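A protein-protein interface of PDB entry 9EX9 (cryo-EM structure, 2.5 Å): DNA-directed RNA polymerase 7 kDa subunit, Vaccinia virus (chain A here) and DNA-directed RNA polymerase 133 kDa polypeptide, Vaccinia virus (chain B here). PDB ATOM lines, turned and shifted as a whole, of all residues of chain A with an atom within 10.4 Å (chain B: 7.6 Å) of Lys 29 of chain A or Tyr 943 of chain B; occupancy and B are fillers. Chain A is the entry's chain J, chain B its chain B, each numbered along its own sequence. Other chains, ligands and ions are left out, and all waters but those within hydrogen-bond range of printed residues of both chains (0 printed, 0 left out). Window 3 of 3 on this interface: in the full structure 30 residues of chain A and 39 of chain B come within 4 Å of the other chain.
Tyr 943 of chain B touches just one residue of chain A: Lys 29 (3.3 Å). No residue of chain A comes within 4 Å of Lys 941 of chain B. No residue of chain A comes within 4 Å of Asn 944 of chain B. Gly 947 of chain B touches one residue of chain A. Printed residues of chain A within 4 Å of Ser 939 of chain B: Arg 41 (2.8 Å). Of the printed residues of chain B, Leu 32 of chain A touches Pro 942 (3.6 Å). Of the printed residues of chain B, Leu 42 of chain A touches Tyr 938. Leu 21 of chain A touches none of the printed residues of chain B. The nearest residue of chain B that does not touch Lys 29 of chain A is His 975 of chain B (4.3 Å).
The backbone carbonyl oxygen (O) of Ser 939 of chain B sits at hydrogen-bond distance from the guanidinium group (NE) of Arg 41 of chain A (2.8 Å). The guanidinium group of Arg 41 of chain A lies within hydrogen-bond range of the backbone carbonyl oxygen of Ala 940 of chain B, at 3.2 Å. The side-chain hydroxyl (OH) of Tyr 943 of chain B lies within hydrogen-bond range of the side-chain amino group (NZ) of Lys 29 of chain A (3.3 Å). The backbone carbonyl oxygen (O) of Gly 947 of chain B is in hydrogen-bond range of the side-chain hydroxyl (OG) of Ser 27 of chain A (3.5 Å). The side-chain amide nitrogen of Asn 949 of chain B lies within hydrogen-bond range of the backbone carbonyl oxygen of Ser 45 of chain A, 3.4 Å away.
The side-chain amide oxygen (OD1) of Asn 949 of chain B lies within hydrogen-bond range of the side-chain hydroxyl (OH) of Tyr 938 of chain B (2.6 Å). O of Ala 940 of chain B is in hydrogen-bond range of OG of Ser 976 of chain B (3.0 Å). The side-chain amino group of Lys 941 of chain B is in hydrogen-bond range of the backbone carbonyl oxygen of Tyr 943 of chain B. O of Pro 942 of chain B lies within hydrogen-bond range of N of Arg 950 of chain B, at 3.2 Å. The side-chain hydroxyl of Ser 27 of chain A lies close to the backbone NH of Lys 29 of chain A (3.4 Å). The guanidinium group (NH1) of Arg 41 of chain A lies within hydrogen-bond range of the backbone carbonyl oxygen (O) of Val 35 of chain A (2.9 Å).
Of the 18 printed residues of chain B, 7 touch a printed residue of chain A. Hydrophobic or aromatic side chains of chain B within 4 Å of the printed part of chain A: Tyr 938, Pro 942 and Tyr 943. Of the 19 printed residues of chain A, 6 touch a printed residue of chain B. Hydrophobic or aromatic side chains of chain A within 4 Å of the printed part of chain B: Leu 32 and Leu 42. Among the printed residues, 8 pairs touch across the chains. Among the printed residues, no Asp or Glu carboxylate lies within 4 Å of a Lys or Arg side-chain nitrogen of the other chain.
CD1 of Leu 32 of chain A touches CG of Pro 942 of chain B (3.6 Å). Tyr 938 of chain B touches Leu 42 of chain A. OH of Tyr 938 of chain B touches CB of Ser 45 of chain A, 3.9 Å away.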
ATOM      1  N   GLU A  17     -20.274  -3.597   4.671  1.00  0.00           N
ATOM      2  CA  GLU A  17     -20.957  -2.364   5.040  1.00  0.00           C
ATOM      3  C   GLU A  17     -21.150  -2.277   6.546  1.00  0.00           C
ATOM      4  O   GLU A  17     -21.047  -1.196   7.132  1.00  0.00           O
ATOM      5  CB  GLU A  17     -22.299  -2.271   4.318  1.00  0.00           C
ATOM      6  CG  GLU A  17     -22.199  -1.819   2.873  1.00  0.00           C
ATOM      7  CD  GLU A  17     -21.685  -2.897   1.949  1.00  0.00           C
ATOM      8  OE1 GLU A  17     -21.594  -4.061   2.381  1.00  0.00           O
ATOM      9  OE2 GLU A  17     -21.373  -2.584   0.784  1.00  0.00           O
ATOM     10  N   LYS A  20     -18.001  -1.095   7.952  1.00  0.00           N
ATOM     11  CA  LYS A  20     -17.819   0.309   7.603  1.00  0.00           C
ATOM     12  C   LYS A  20     -18.673   1.215   8.474  1.00  0.00           C
ATOM     13  O   LYS A  20     -18.296   2.362   8.731  1.00  0.00           O
ATOM     14  CB  LYS A  20     -18.158   0.515   6.128  1.00  0.00           C
ATOM     15  CG  LYS A  20     -17.858   1.895   5.600  1.00  0.00           C
ATOM     16  CD  LYS A  20     -18.192   1.989   4.125  1.00  0.00           C
ATOM     17  CE  LYS A  20     -17.870   3.358   3.558  1.00  0.00           C
ATOM     18  NZ  LYS A  20     -18.169   3.439   2.105  1.00  0.00           N
ATOM     19  N   LEU A  21     -19.820   0.725   8.934  1.00  0.00           N
ATOM     20  CA  LEU A  21     -20.723   1.550   9.729  1.00  0.00           C
ATOM     21  C   LEU A  21     -20.367   1.516  11.211  1.00  0.00           C
ATOM     22  O   LEU A  21     -20.257   2.565  11.852  1.00  0.00           O
ATOM     23  CB  LEU A  21     -22.161   1.081   9.526  1.00  0.00           C
ATOM     24  CG  LEU A  21     -23.245   1.867  10.258  1.00  0.00           C
ATOM     25  CD1 LEU A  21     -23.429   3.226   9.624  1.00  0.00           C
ATOM     26  CD2 LEU A  21     -24.543   1.097  10.255  1.00  0.00           C
ATOM     27  N   LYS A  25     -17.439   4.076  11.810  1.00  0.00           N
ATOM     28  CA  LYS A  25     -18.396   5.122  12.153  1.00  0.00           C
ATOM     29  C   LYS A  25     -18.492   6.167  11.048  1.00  0.00           C
ATOM     30  O   LYS A  25     -18.387   7.371  11.282  1.00  0.00           O
ATOM     31  CB  LYS A  25     -18.030   5.767  13.486  1.00  0.00           C
ATOM     32  CG  LYS A  25     -18.130   4.817  14.654  1.00  0.00           C
ATOM     33  CD  LYS A  25     -17.666   5.469  15.932  1.00  0.00           C
ATOM     34  CE  LYS A  25     -17.716   4.502  17.094  1.00  0.00           C
ATOM     35  NZ  LYS A  25     -17.210   5.126  18.344  1.00  0.00           N
ATOM     36  N   LYS A  26     -18.680   5.691   9.824  1.00  0.00           N
ATOM     37  CA  LYS A  26     -18.986   6.566   8.708  1.00  0.00           C
ATOM     38  C   LYS A  26     -20.461   6.950   8.734  1.00  0.00           C
ATOM     39  O   LYS A  26     -21.272   6.375   9.462  1.00  0.00           O
ATOM     40  CB  LYS A  26     -18.642   5.886   7.389  1.00  0.00           C
ATOM     41  CG  LYS A  26     -17.171   5.636   7.193  1.00  0.00           C
ATOM     42  CD  LYS A  26     -16.428   6.928   6.964  1.00  0.00           C
ATOM     43  CE  LYS A  26     -14.968   6.673   6.673  1.00  0.00           C
ATOM     44  NZ  LYS A  26     -14.786   5.864   5.441  1.00  0.00           N
ATOM     45  N   SER A  27     -20.807   7.946   7.928  1.00  0.00           N
ATOM     46  CA  SER A  27     -22.190   8.378   7.838  1.00  0.00           C
ATOM     47  C   SER A  27     -23.047   7.286   7.214  1.00  0.00           C
ATOM     48  O   SER A  27     -22.589   6.505   6.379  1.00  0.00           O
ATOM     49  CB  SER A  27     -22.293   9.656   7.012  1.00  0.00           C
ATOM     50  OG  SER A  27     -23.639  10.060   6.867  1.00  0.00           O
ATOM     51  N   LEU A  28     -24.311   7.230   7.635  1.00  0.00           N
ATOM     52  CA  LEU A  28     -25.225   6.243   7.075  1.00  0.00           C
ATOM     53  C   LEU A  28     -25.389   6.440   5.572  1.00  0.00           C
ATOM     54  O   LEU A  28     -25.554   5.471   4.825  1.00  0.00           O
ATOM     55  CB  LEU A  28     -26.573   6.329   7.784  1.00  0.00           C
ATOM     56  CG  LEU A  28     -27.620   5.281   7.424  1.00  0.00           C
ATOM     57  CD1 LEU A  28     -27.145   3.896   7.798  1.00  0.00           C
ATOM     58  CD2 LEU A  28     -28.922   5.599   8.115  1.00  0.00           C
ATOM     59  N   LYS A  29     -25.336   7.690   5.110  1.00  0.00           N
ATOM     60  CA  LYS A  29     -25.420   7.963   3.680  1.00  0.00           C
ATOM     61  C   LYS A  29     -24.238   7.353   2.932  1.00  0.00           C
ATOM     62  O   LYS A  29     -24.413   6.653   1.924  1.00  0.00           O
ATOM     63  CB  LYS A  29     -25.483   9.474   3.464  1.00  0.00           C
ATOM     64  CG  LYS A  29     -25.503   9.922   2.020  1.00  0.00           C
ATOM     65  CD  LYS A  29     -25.548  11.437   1.940  1.00  0.00           C
ATOM     66  CE  LYS A  29     -25.532  11.934   0.505  1.00  0.00           C
ATOM     67  NZ  LYS A  29     -26.735  11.511  -0.258  1.00  0.00           N
ATOM     68  N   ASP A  30     -23.022   7.602   3.419  1.00  0.00           N
ATOM     69  CA  ASP A  30     -21.840   7.064   2.757  1.00  0.00           C
ATOM     70  C   ASP A  30     -21.856   5.546   2.763  1.00  0.00           C
ATOM     71  O   ASP A  30     -21.450   4.910   1.786  1.00  0.00           O
ATOM     72  CB  ASP A  30     -20.575   7.582   3.435  1.00  0.00           C
ATOM     73  CG  ASP A  30     -20.469   9.089   3.399  1.00  0.00           C
ATOM     74  OD1 ASP A  30     -21.160   9.716   2.570  1.00  0.00           O
ATOM     75  OD2 ASP A  30     -19.687   9.649   4.193  1.00  0.00           O
ATOM     76  N   VAL A  31     -22.309   4.945   3.863  1.00  0.00           N
ATOM     77  CA  VAL A  31     -22.387   3.491   3.932  1.00  0.00           C
ATOM     78  C   VAL A  31     -23.373   2.964   2.900  1.00  0.00           C
ATOM     79  O   VAL A  31     -23.053   2.069   2.111  1.00  0.00           O
ATOM     80  CB  VAL A  31     -22.765   3.047   5.356  1.00  0.00           C
ATOM     81  CG1 VAL A  31     -23.121   1.573   5.382  1.00  0.00           C
ATOM     82  CG2 VAL A  31     -21.626   3.334   6.304  1.00  0.00           C
ATOM     83  N   LEU A  32     -24.579   3.528   2.870  1.00  0.00           N
ATOM     84  CA  LEU A  32     -25.609   3.022   1.974  1.00  0.00           C
ATOM     85  C   LEU A  32     -25.343   3.348   0.512  1.00  0.00           C
ATOM     86  O   LEU A  32     -26.061   2.836  -0.351  1.00  0.00           O
ATOM     87  CB  LEU A  32     -26.974   3.584   2.369  1.00  0.00           C
ATOM     88  CG  LEU A  32     -27.543   3.148   3.712  1.00  0.00           C
ATOM     89  CD1 LEU A  32     -28.914   3.744   3.907  1.00  0.00           C
ATOM     90  CD2 LEU A  32     -27.602   1.644   3.806  1.00  0.00           C
ATOM     91  N   VAL A  33     -24.358   4.193   0.210  1.00  0.00           N
ATOM     92  CA  VAL A  33     -24.095   4.536  -1.188  1.00  0.00           C
ATOM     93  C   VAL A  33     -24.027   3.305  -2.085  1.00  0.00           C
ATOM     94  O   VAL A  33     -24.325   3.390  -3.282  1.00  0.00           O
ATOM     95  CB  VAL A  33     -22.800   5.362  -1.300  1.00  0.00           C
ATOM     96  CG1 VAL A  33     -21.587   4.468  -1.170  1.00  0.00           C
ATOM     97  CG2 VAL A  33     -22.766   6.101  -2.617  1.00  0.00           C
ATOM     98  N   SER A  34     -23.630   2.151  -1.546  1.00  0.00           N
ATOM     99  CA  SER A  34     -23.411   0.956  -2.356  1.00  0.00           C
ATOM    100  C   SER A  34     -24.392  -0.171  -2.036  1.00  0.00           C
ATOM    101  O   SER A  34     -24.081  -1.337  -2.284  1.00  0.00           O
ATOM    102  CB  SER A  34     -21.977   0.459  -2.189  1.00  0.00           C
ATOM    103  OG  SER A  34     -21.744   0.015  -0.870  1.00  0.00           O
ATOM    104  N   VAL A  35     -25.563   0.151  -1.499  1.00  0.00           N
ATOM    105  CA  VAL A  35     -26.604  -0.827  -1.206  1.00  0.00           C
ATOM    106  C   VAL A  35     -27.879  -0.366  -1.890  1.00  0.00           C
ATOM    107  O   VAL A  35     -28.294   0.783  -1.719  1.00  0.00           O
ATOM    108  CB  VAL A  35     -26.823  -0.984   0.308  1.00  0.00           C
ATOM    109  CG1 VAL A  35     -27.862  -2.044   0.588  1.00  0.00           C
ATOM    110  CG2 VAL A  35     -25.523  -1.323   0.987  1.00  0.00           C
ATOM    111  N   LYS A  36     -28.503  -1.260  -2.651  1.00  0.00           N
ATOM    112  CA  LYS A  36     -29.644  -0.910  -3.488  1.00  0.00           C
ATOM    113  C   LYS A  36     -30.962  -1.497  -3.016  1.00  0.00           C
ATOM    114  O   LYS A  36     -31.987  -0.823  -3.093  1.00  0.00           O
ATOM    115  CB  LYS A  36     -29.390  -1.365  -4.927  1.00  0.00           C
ATOM    116  CG  LYS A  36     -30.551  -1.115  -5.869  1.00  0.00           C
ATOM    117  CD  LYS A  36     -30.179  -1.434  -7.302  1.00  0.00           C
ATOM    118  CE  LYS A  36     -31.327  -1.136  -8.248  1.00  0.00           C
ATOM    119  NZ  LYS A  36     -30.956  -1.373  -9.669  1.00  0.00           N
ATOM    120  N   ARG A  41     -31.135  -2.129   2.934  1.00  0.00           N
ATOM    121  CA  ARG A  41     -31.036  -0.810   3.545  1.00  0.00           C
ATOM    122  C   ARG A  41     -31.701  -0.793   4.913  1.00  0.00           C
ATOM    123  O   ARG A  41     -31.136  -0.273   5.882  1.00  0.00           O
ATOM    124  CB  ARG A  41     -31.660   0.233   2.622  1.00  0.00           C
ATOM    125  CG  ARG A  41     -30.951   0.354   1.291  1.00  0.00           C
ATOM    126  CD  ARG A  41     -31.752   1.150   0.291  1.00  0.00           C
ATOM    127  NE  ARG A  41     -31.744   2.577   0.579  1.00  0.00           N
ATOM    128  CZ  ARG A  41     -30.792   3.414   0.195  1.00  0.00           C
ATOM    129  NH1 ARG A  41     -29.728   2.995  -0.467  1.00  0.00           N
ATOM    130  NH2 ARG A  41     -30.910   4.704   0.481  1.00  0.00           N
ATOM    131  N   LEU A  42     -32.892  -1.381   5.021  1.00  0.00           N
ATOM    132  CA  LEU A  42     -33.557  -1.409   6.318  1.00  0.00           C
ATOM    133  C   LEU A  42     -32.746  -2.200   7.335  1.00  0.00           C
ATOM    134  O   LEU A  42     -32.634  -1.796   8.499  1.00  0.00           O
ATOM    135  CB  LEU A  42     -34.958  -1.997   6.187  1.00  0.00           C
ATOM    136  CG  LEU A  42     -36.080  -1.041   5.791  1.00  0.00           C
ATOM    137  CD1 LEU A  42     -37.378  -1.799   5.669  1.00  0.00           C
ATOM    138  CD2 LEU A  42     -36.231   0.075   6.798  1.00  0.00           C
ATOM    139  N   LEU A  44     -29.452  -2.722   7.454  1.00  0.00           N
ATOM    140  CA  LEU A  44     -28.277  -1.978   7.881  1.00  0.00           C
ATOM    141  C   LEU A  44     -28.635  -0.746   8.695  1.00  0.00           C
ATOM    142  O   LEU A  44     -27.792  -0.260   9.453  1.00  0.00           O
ATOM    143  CB  LEU A  44     -27.439  -1.575   6.674  1.00  0.00           C
ATOM    144  CG  LEU A  44     -26.521  -2.669   6.137  1.00  0.00           C
ATOM    145  CD1 LEU A  44     -25.979  -2.272   4.785  1.00  0.00           C
ATOM    146  CD2 LEU A  44     -25.384  -2.942   7.100  1.00  0.00           C
ATOM    147  N   SER A  45     -29.856  -0.227   8.562  1.00  0.00           N
ATOM    148  CA  SER A  45     -30.242   0.966   9.304  1.00  0.00           C
ATOM    149  C   SER A  45     -30.876   0.681  10.660  1.00  0.00           C
ATOM    150  O   SER A  45     -30.807   1.543  11.540  1.00  0.00           O
ATOM    151  CB  SER A  45     -31.218   1.804   8.479  1.00  0.00           C
ATOM    152  OG  SER A  45     -30.649   2.163   7.239  1.00  0.00           O
ATOM    153  N   ALA B 937     -40.904   4.591   2.413  1.00  0.00           N
ATOM    154  CA  ALA B 937     -40.249   5.880   2.255  1.00  0.00           C
ATOM    155  C   ALA B 937     -38.981   5.940   3.089  1.00  0.00           C
ATOM    156  O   ALA B 937     -37.937   6.393   2.612  1.00  0.00           O
ATOM    157  CB  ALA B 937     -41.206   7.005   2.637  1.00  0.00           C
ATOM    158  N   TYR B 938     -39.037   5.441   4.327  1.00  0.00           N
ATOM    159  CA  TYR B 938     -37.849   5.489   5.165  1.00  0.00           C
ATOM    160  C   TYR B 938     -36.699   4.736   4.527  1.00  0.00           C
ATOM    161  O   TYR B 938     -35.537   5.115   4.701  1.00  0.00           O
ATOM    162  CB  TYR B 938     -38.130   4.913   6.548  1.00  0.00           C
ATOM    163  CG  TYR B 938     -36.890   4.866   7.411  1.00  0.00           C
ATOM    164  CD1 TYR B 938     -36.030   3.780   7.367  1.00  0.00           C
ATOM    165  CD2 TYR B 938     -36.567   5.913   8.254  1.00  0.00           C
ATOM    166  CE1 TYR B 938     -34.895   3.739   8.138  1.00  0.00           C
ATOM    167  CE2 TYR B 938     -35.434   5.876   9.030  1.00  0.00           C
ATOM    168  CZ  TYR B 938     -34.603   4.788   8.968  1.00  0.00           C
ATOM    169  OH  TYR B 938     -33.471   4.744   9.742  1.00  0.00           O
ATOM    170  N   SER B 939     -36.993   3.663   3.797  1.00  0.00           N
ATOM    171  CA  SER B 939     -35.917   2.891   3.199  1.00  0.00           C
ATOM    172  C   SER B 939     -35.269   3.648   2.057  1.00  0.00           C
ATOM    173  O   SER B 939     -34.084   3.445   1.777  1.00  0.00           O
ATOM    174  CB  SER B 939     -36.446   1.547   2.714  1.00  0.00           C
ATOM    175  OG  SER B 939     -35.386   0.738   2.253  1.00  0.00           O
ATOM    176  N   ALA B 940     -36.019   4.524   1.390  1.00  0.00           N
ATOM    177  CA  ALA B 940     -35.456   5.253   0.261  1.00  0.00           C
ATOM    178  C   ALA B 940     -34.529   6.367   0.729  1.00  0.00           C
ATOM    179  O   ALA B 940     -33.498   6.627   0.102  1.00  0.00           O
ATOM    180  CB  ALA B 940     -36.577   5.813  -0.605  1.00  0.00           C
ATOM    181  N   LYS B 941     -34.878   7.035   1.828  1.00  0.00           N
ATOM    182  CA  LYS B 941     -34.073   8.135   2.357  1.00  0.00           C
ATOM    183  C   LYS B 941     -34.156   8.091   3.870  1.00  0.00           C
ATOM    184  O   LYS B 941     -35.006   8.750   4.480  1.00  0.00           O
ATOM    185  CB  LYS B 941     -34.551   9.486   1.832  1.00  0.00           C
ATOM    186  CG  LYS B 941     -33.718  10.660   2.300  1.00  0.00           C
ATOM    187  CD  LYS B 941     -34.218  11.961   1.707  1.00  0.00           C
ATOM    188  CE  LYS B 941     -33.240  13.093   1.945  1.00  0.00           C
ATOM    189  NZ  LYS B 941     -33.021  13.361   3.385  1.00  0.00           N
ATOM    190  N   PRO B 942     -33.294   7.310   4.518  1.00  0.00           N
ATOM    191  CA  PRO B 942     -33.378   7.136   5.974  1.00  0.00           C
ATOM    192  C   PRO B 942     -32.593   8.139   6.808  1.00  0.00           C
ATOM    193  O   PRO B 942     -32.390   7.882   7.997  1.00  0.00           O
ATOM    194  CB  PRO B 942     -32.802   5.727   6.158  1.00  0.00           C
ATOM    195  CG  PRO B 942     -31.808   5.595   5.079  1.00  0.00           C
ATOM    196  CD  PRO B 942     -32.327   6.378   3.912  1.00  0.00           C
ATOM    197  N   TYR B 943     -32.149   9.261   6.249  1.00  0.00           N
ATOM    198  CA  TYR B 943     -31.293  10.192   6.966  1.00  0.00           C
ATOM    199  C   TYR B 943     -31.748  11.626   6.746  1.00  0.00           C
ATOM    200  O   TYR B 943     -32.384  11.956   5.744  1.00  0.00           O
ATOM    201  CB  TYR B 943     -29.833  10.040   6.535  1.00  0.00           C
ATOM    202  CG  TYR B 943     -29.656   9.938   5.045  1.00  0.00           C
ATOM    203  CD1 TYR B 943     -29.744  11.058   4.238  1.00  0.00           C
ATOM    204  CD2 TYR B 943     -29.401   8.719   4.443  1.00  0.00           C
ATOM    205  CE1 TYR B 943     -29.585  10.968   2.876  1.00  0.00           C
ATOM    206  CE2 TYR B 943     -29.244   8.619   3.080  1.00  0.00           C
ATOM    207  CZ  TYR B 943     -29.335   9.746   2.303  1.00  0.00           C
ATOM    208  OH  TYR B 943     -29.175   9.646   0.943  1.00  0.00           O
ATOM    209  N   ASN B 944     -31.401  12.478   7.709  1.00  0.00           N
ATOM    210  CA  ASN B 944     -31.683  13.904   7.645  1.00  0.00           C
ATOM    211  C   ASN B 944     -30.840  14.564   6.562  1.00  0.00           C
ATOM    212  O   ASN B 944     -30.032  13.926   5.885  1.00  0.00           O
ATOM    213  CB  ASN B 944     -31.388  14.562   8.992  1.00  0.00           C
ATOM    214  CG  ASN B 944     -32.558  14.511   9.938  1.00  0.00           C
ATOM    215  OD1 ASN B 944     -33.708  14.612   9.522  1.00  0.00           O
ATOM    216  ND2 ASN B 944     -32.271  14.368  11.226  1.00  0.00           N
ATOM    217  N   ASN B 945     -31.027  15.873   6.404  1.00  0.00           N
ATOM    218  CA  ASN B 945     -30.135  16.649   5.553  1.00  0.00           C
ATOM    219  C   ASN B 945     -28.753  16.799   6.170  1.00  0.00           C
ATOM    220  O   ASN B 945     -27.822  17.221   5.479  1.00  0.00           O
ATOM    221  CB  ASN B 945     -30.737  18.022   5.277  1.00  0.00           C
ATOM    222  CG  ASN B 945     -32.042  17.936   4.521  1.00  0.00           C
ATOM    223  OD1 ASN B 945     -33.116  17.888   5.117  1.00  0.00           O
ATOM    224  ND2 ASN B 945     -31.956  17.903   3.198  1.00  0.00           N
ATOM    225  N   LYS B 946     -28.603  16.475   7.450  1.00  0.00           N
ATOM    226  CA  LYS B 946     -27.302  16.413   8.096  1.00  0.00           C
ATOM    227  C   LYS B 946     -26.682  15.024   8.031  1.00  0.00           C
ATOM    228  O   LYS B 946     -25.531  14.856   8.445  1.00  0.00           O
ATOM    229  CB  LYS B 946     -27.425  16.849   9.556  1.00  0.00           C
ATOM    230  CG  LYS B 946     -28.095  18.196   9.738  1.00  0.00           C
ATOM    231  CD  LYS B 946     -28.227  18.551  11.204  1.00  0.00           C
ATOM    232  CE  LYS B 946     -28.931  19.884  11.391  1.00  0.00           C
ATOM    233  NZ  LYS B 946     -29.084  20.229  12.832  1.00  0.00           N
ATOM    234  N   GLY B 947     -27.408  14.033   7.518  1.00  0.00           N
ATOM    235  CA  GLY B 947     -26.898  12.684   7.414  1.00  0.00           C
ATOM    236  C   GLY B 947     -27.116  11.816   8.630  1.00  0.00           C
ATOM    237  O   GLY B 947     -26.475  10.766   8.739  1.00  0.00           O
ATOM    238  N   GLU B 948     -27.991  12.217   9.546  1.00  0.00           N
ATOM    239  CA  GLU B 948     -28.262  11.444  10.749  1.00  0.00           C
ATOM    240  C   GLU B 948     -29.501  10.583  10.556  1.00  0.00           C
ATOM    241  O   GLU B 948     -30.452  10.988   9.887  1.00  0.00           O
ATOM    242  CB  GLU B 948     -28.466  12.367  11.947  1.00  0.00           C
ATOM    243  CG  GLU B 948     -27.304  13.291  12.233  1.00  0.00           C
ATOM    244  CD  GLU B 948     -27.672  14.387  13.211  1.00  0.00           C
ATOM    245  OE1 GLU B 948     -28.814  14.374  13.714  1.00  0.00           O
ATOM    246  OE2 GLU B 948     -26.823  15.263  13.473  1.00  0.00           O
ATOM    247  N   ASN B 949     -29.488   9.400  11.158  1.00  0.00           N
ATOM    248  CA  ASN B 949     -30.647   8.523  11.094  1.00  0.00           C
ATOM    249  C   ASN B 949     -31.884   9.265  11.583  1.00  0.00           C
ATOM    250  O   ASN B 949     -31.862   9.900  12.638  1.00  0.00           O
ATOM    251  CB  ASN B 949     -30.392   7.282  11.943  1.00  0.00           C
ATOM    252  CG  ASN B 949     -31.416   6.201  11.721  1.00  0.00           C
ATOM    253  OD1 ASN B 949     -32.571   6.477  11.420  1.00  0.00           O
ATOM    254  ND2 ASN B 949     -30.997   4.956  11.876  1.00  0.00           N
ATOM    255  N   ARG B 950     -32.966   9.186  10.812  1.00  0.00           N
ATOM    256  CA  ARG B 950     -34.172   9.975  11.066  1.00  0.00           C
ATOM    257  C   ARG B 950     -35.406   9.084  11.096  1.00  0.00           C
ATOM    258  O   ARG B 950     -35.899   8.672  10.033  1.00  0.00           O
ATOM    259  CB  ARG B 950     -34.327  11.055   9.998  1.00  0.00           C
ATOM    260  CG  ARG B 950     -35.506  11.980  10.208  1.00  0.00           C
ATOM    261  CD  ARG B 950     -36.704  11.627   9.340  1.00  0.00           C
ATOM    262  NE  ARG B 950     -36.474  11.877   7.921  1.00  0.00           N
ATOM    263  CZ  ARG B 950     -36.228  10.945   7.012  1.00  0.00           C
ATOM    264  NH1 ARG B 950     -36.148   9.665   7.332  1.00  0.00           N
ATOM    265  NH2 ARG B 950     -36.064  11.304   5.745  1.00  0.00           N
ATOM    266  N   PRO B 951     -35.941   8.756  12.265  1.00  0.00           N
ATOM    267  CA  PRO B 951     -37.215   8.033  12.312  1.00  0.00           C
ATOM    268  C   PRO B 951     -38.372   8.904  11.847  1.00  0.00           C
ATOM    269  O   PRO B 951     -38.293  10.131  11.810  1.00  0.00           O
ATOM    270  CB  PRO B 951     -37.360   7.661  13.790  1.00  0.00           C
ATOM    271  CG  PRO B 951     -35.989   7.707  14.330  1.00  0.00           C
ATOM    272  CD  PRO B 951     -35.287   8.788  13.580  1.00  0.00           C
ATOM    273  N   CYS B 972     -39.123  11.821  -0.657  1.00  0.00           N
ATOM    274  CA  CYS B 972     -38.095  10.812  -0.421  1.00  0.00           C
ATOM    275  C   CYS B 972     -37.704  10.118  -1.721  1.00  0.00           C
ATOM    276  O   CYS B 972     -36.517  10.025  -2.063  1.00  0.00           O
ATOM    277  CB  CYS B 972     -38.584   9.793   0.605  1.00  0.00           C
ATOM    278  SG  CYS B 972     -38.587  10.383   2.304  1.00  0.00           S
ATOM    279  N   HIS B 975     -35.788  12.393  -4.147  1.00  0.00           N
ATOM    280  CA  HIS B 975     -34.387  12.509  -3.759  1.00  0.00           C
ATOM    281  C   HIS B 975     -33.612  11.266  -4.162  1.00  0.00           C
ATOM    282  O   HIS B 975     -32.486  11.362  -4.663  1.00  0.00           O
ATOM    283  CB  HIS B 975     -34.262  12.734  -2.257  1.00  0.00           C
ATOM    284  CG  HIS B 975     -32.858  12.604  -1.751  1.00  0.00           C
ATOM    285  ND1 HIS B 975     -31.929  13.614  -1.865  1.00  0.00           N
ATOM    286  CD2 HIS B 975     -32.222  11.575  -1.141  1.00  0.00           C
ATOM    287  CE1 HIS B 975     -30.783  13.218  -1.340  1.00  0.00           C
ATOM    288  NE2 HIS B 975     -30.935  11.984  -0.894  1.00  0.00           N
ATOM    289  N   SER B 976     -34.197  10.087  -3.945  1.00  0.00           N
ATOM    290  CA  SER B 976     -33.493   8.846  -4.253  1.00  0.00           C
ATOM    291  C   SER B 976     -33.167   8.748  -5.739  1.00  0.00           C
ATOM    292  O   SER B 976     -31.996   8.695  -6.128  1.00  0.00           O
ATOM    293  CB  SER B 976     -34.331   7.655  -3.801  1.00  0.00           C
ATOM    294  OG  SER B 976     -34.601   7.746  -2.416  1.00  0.00           O
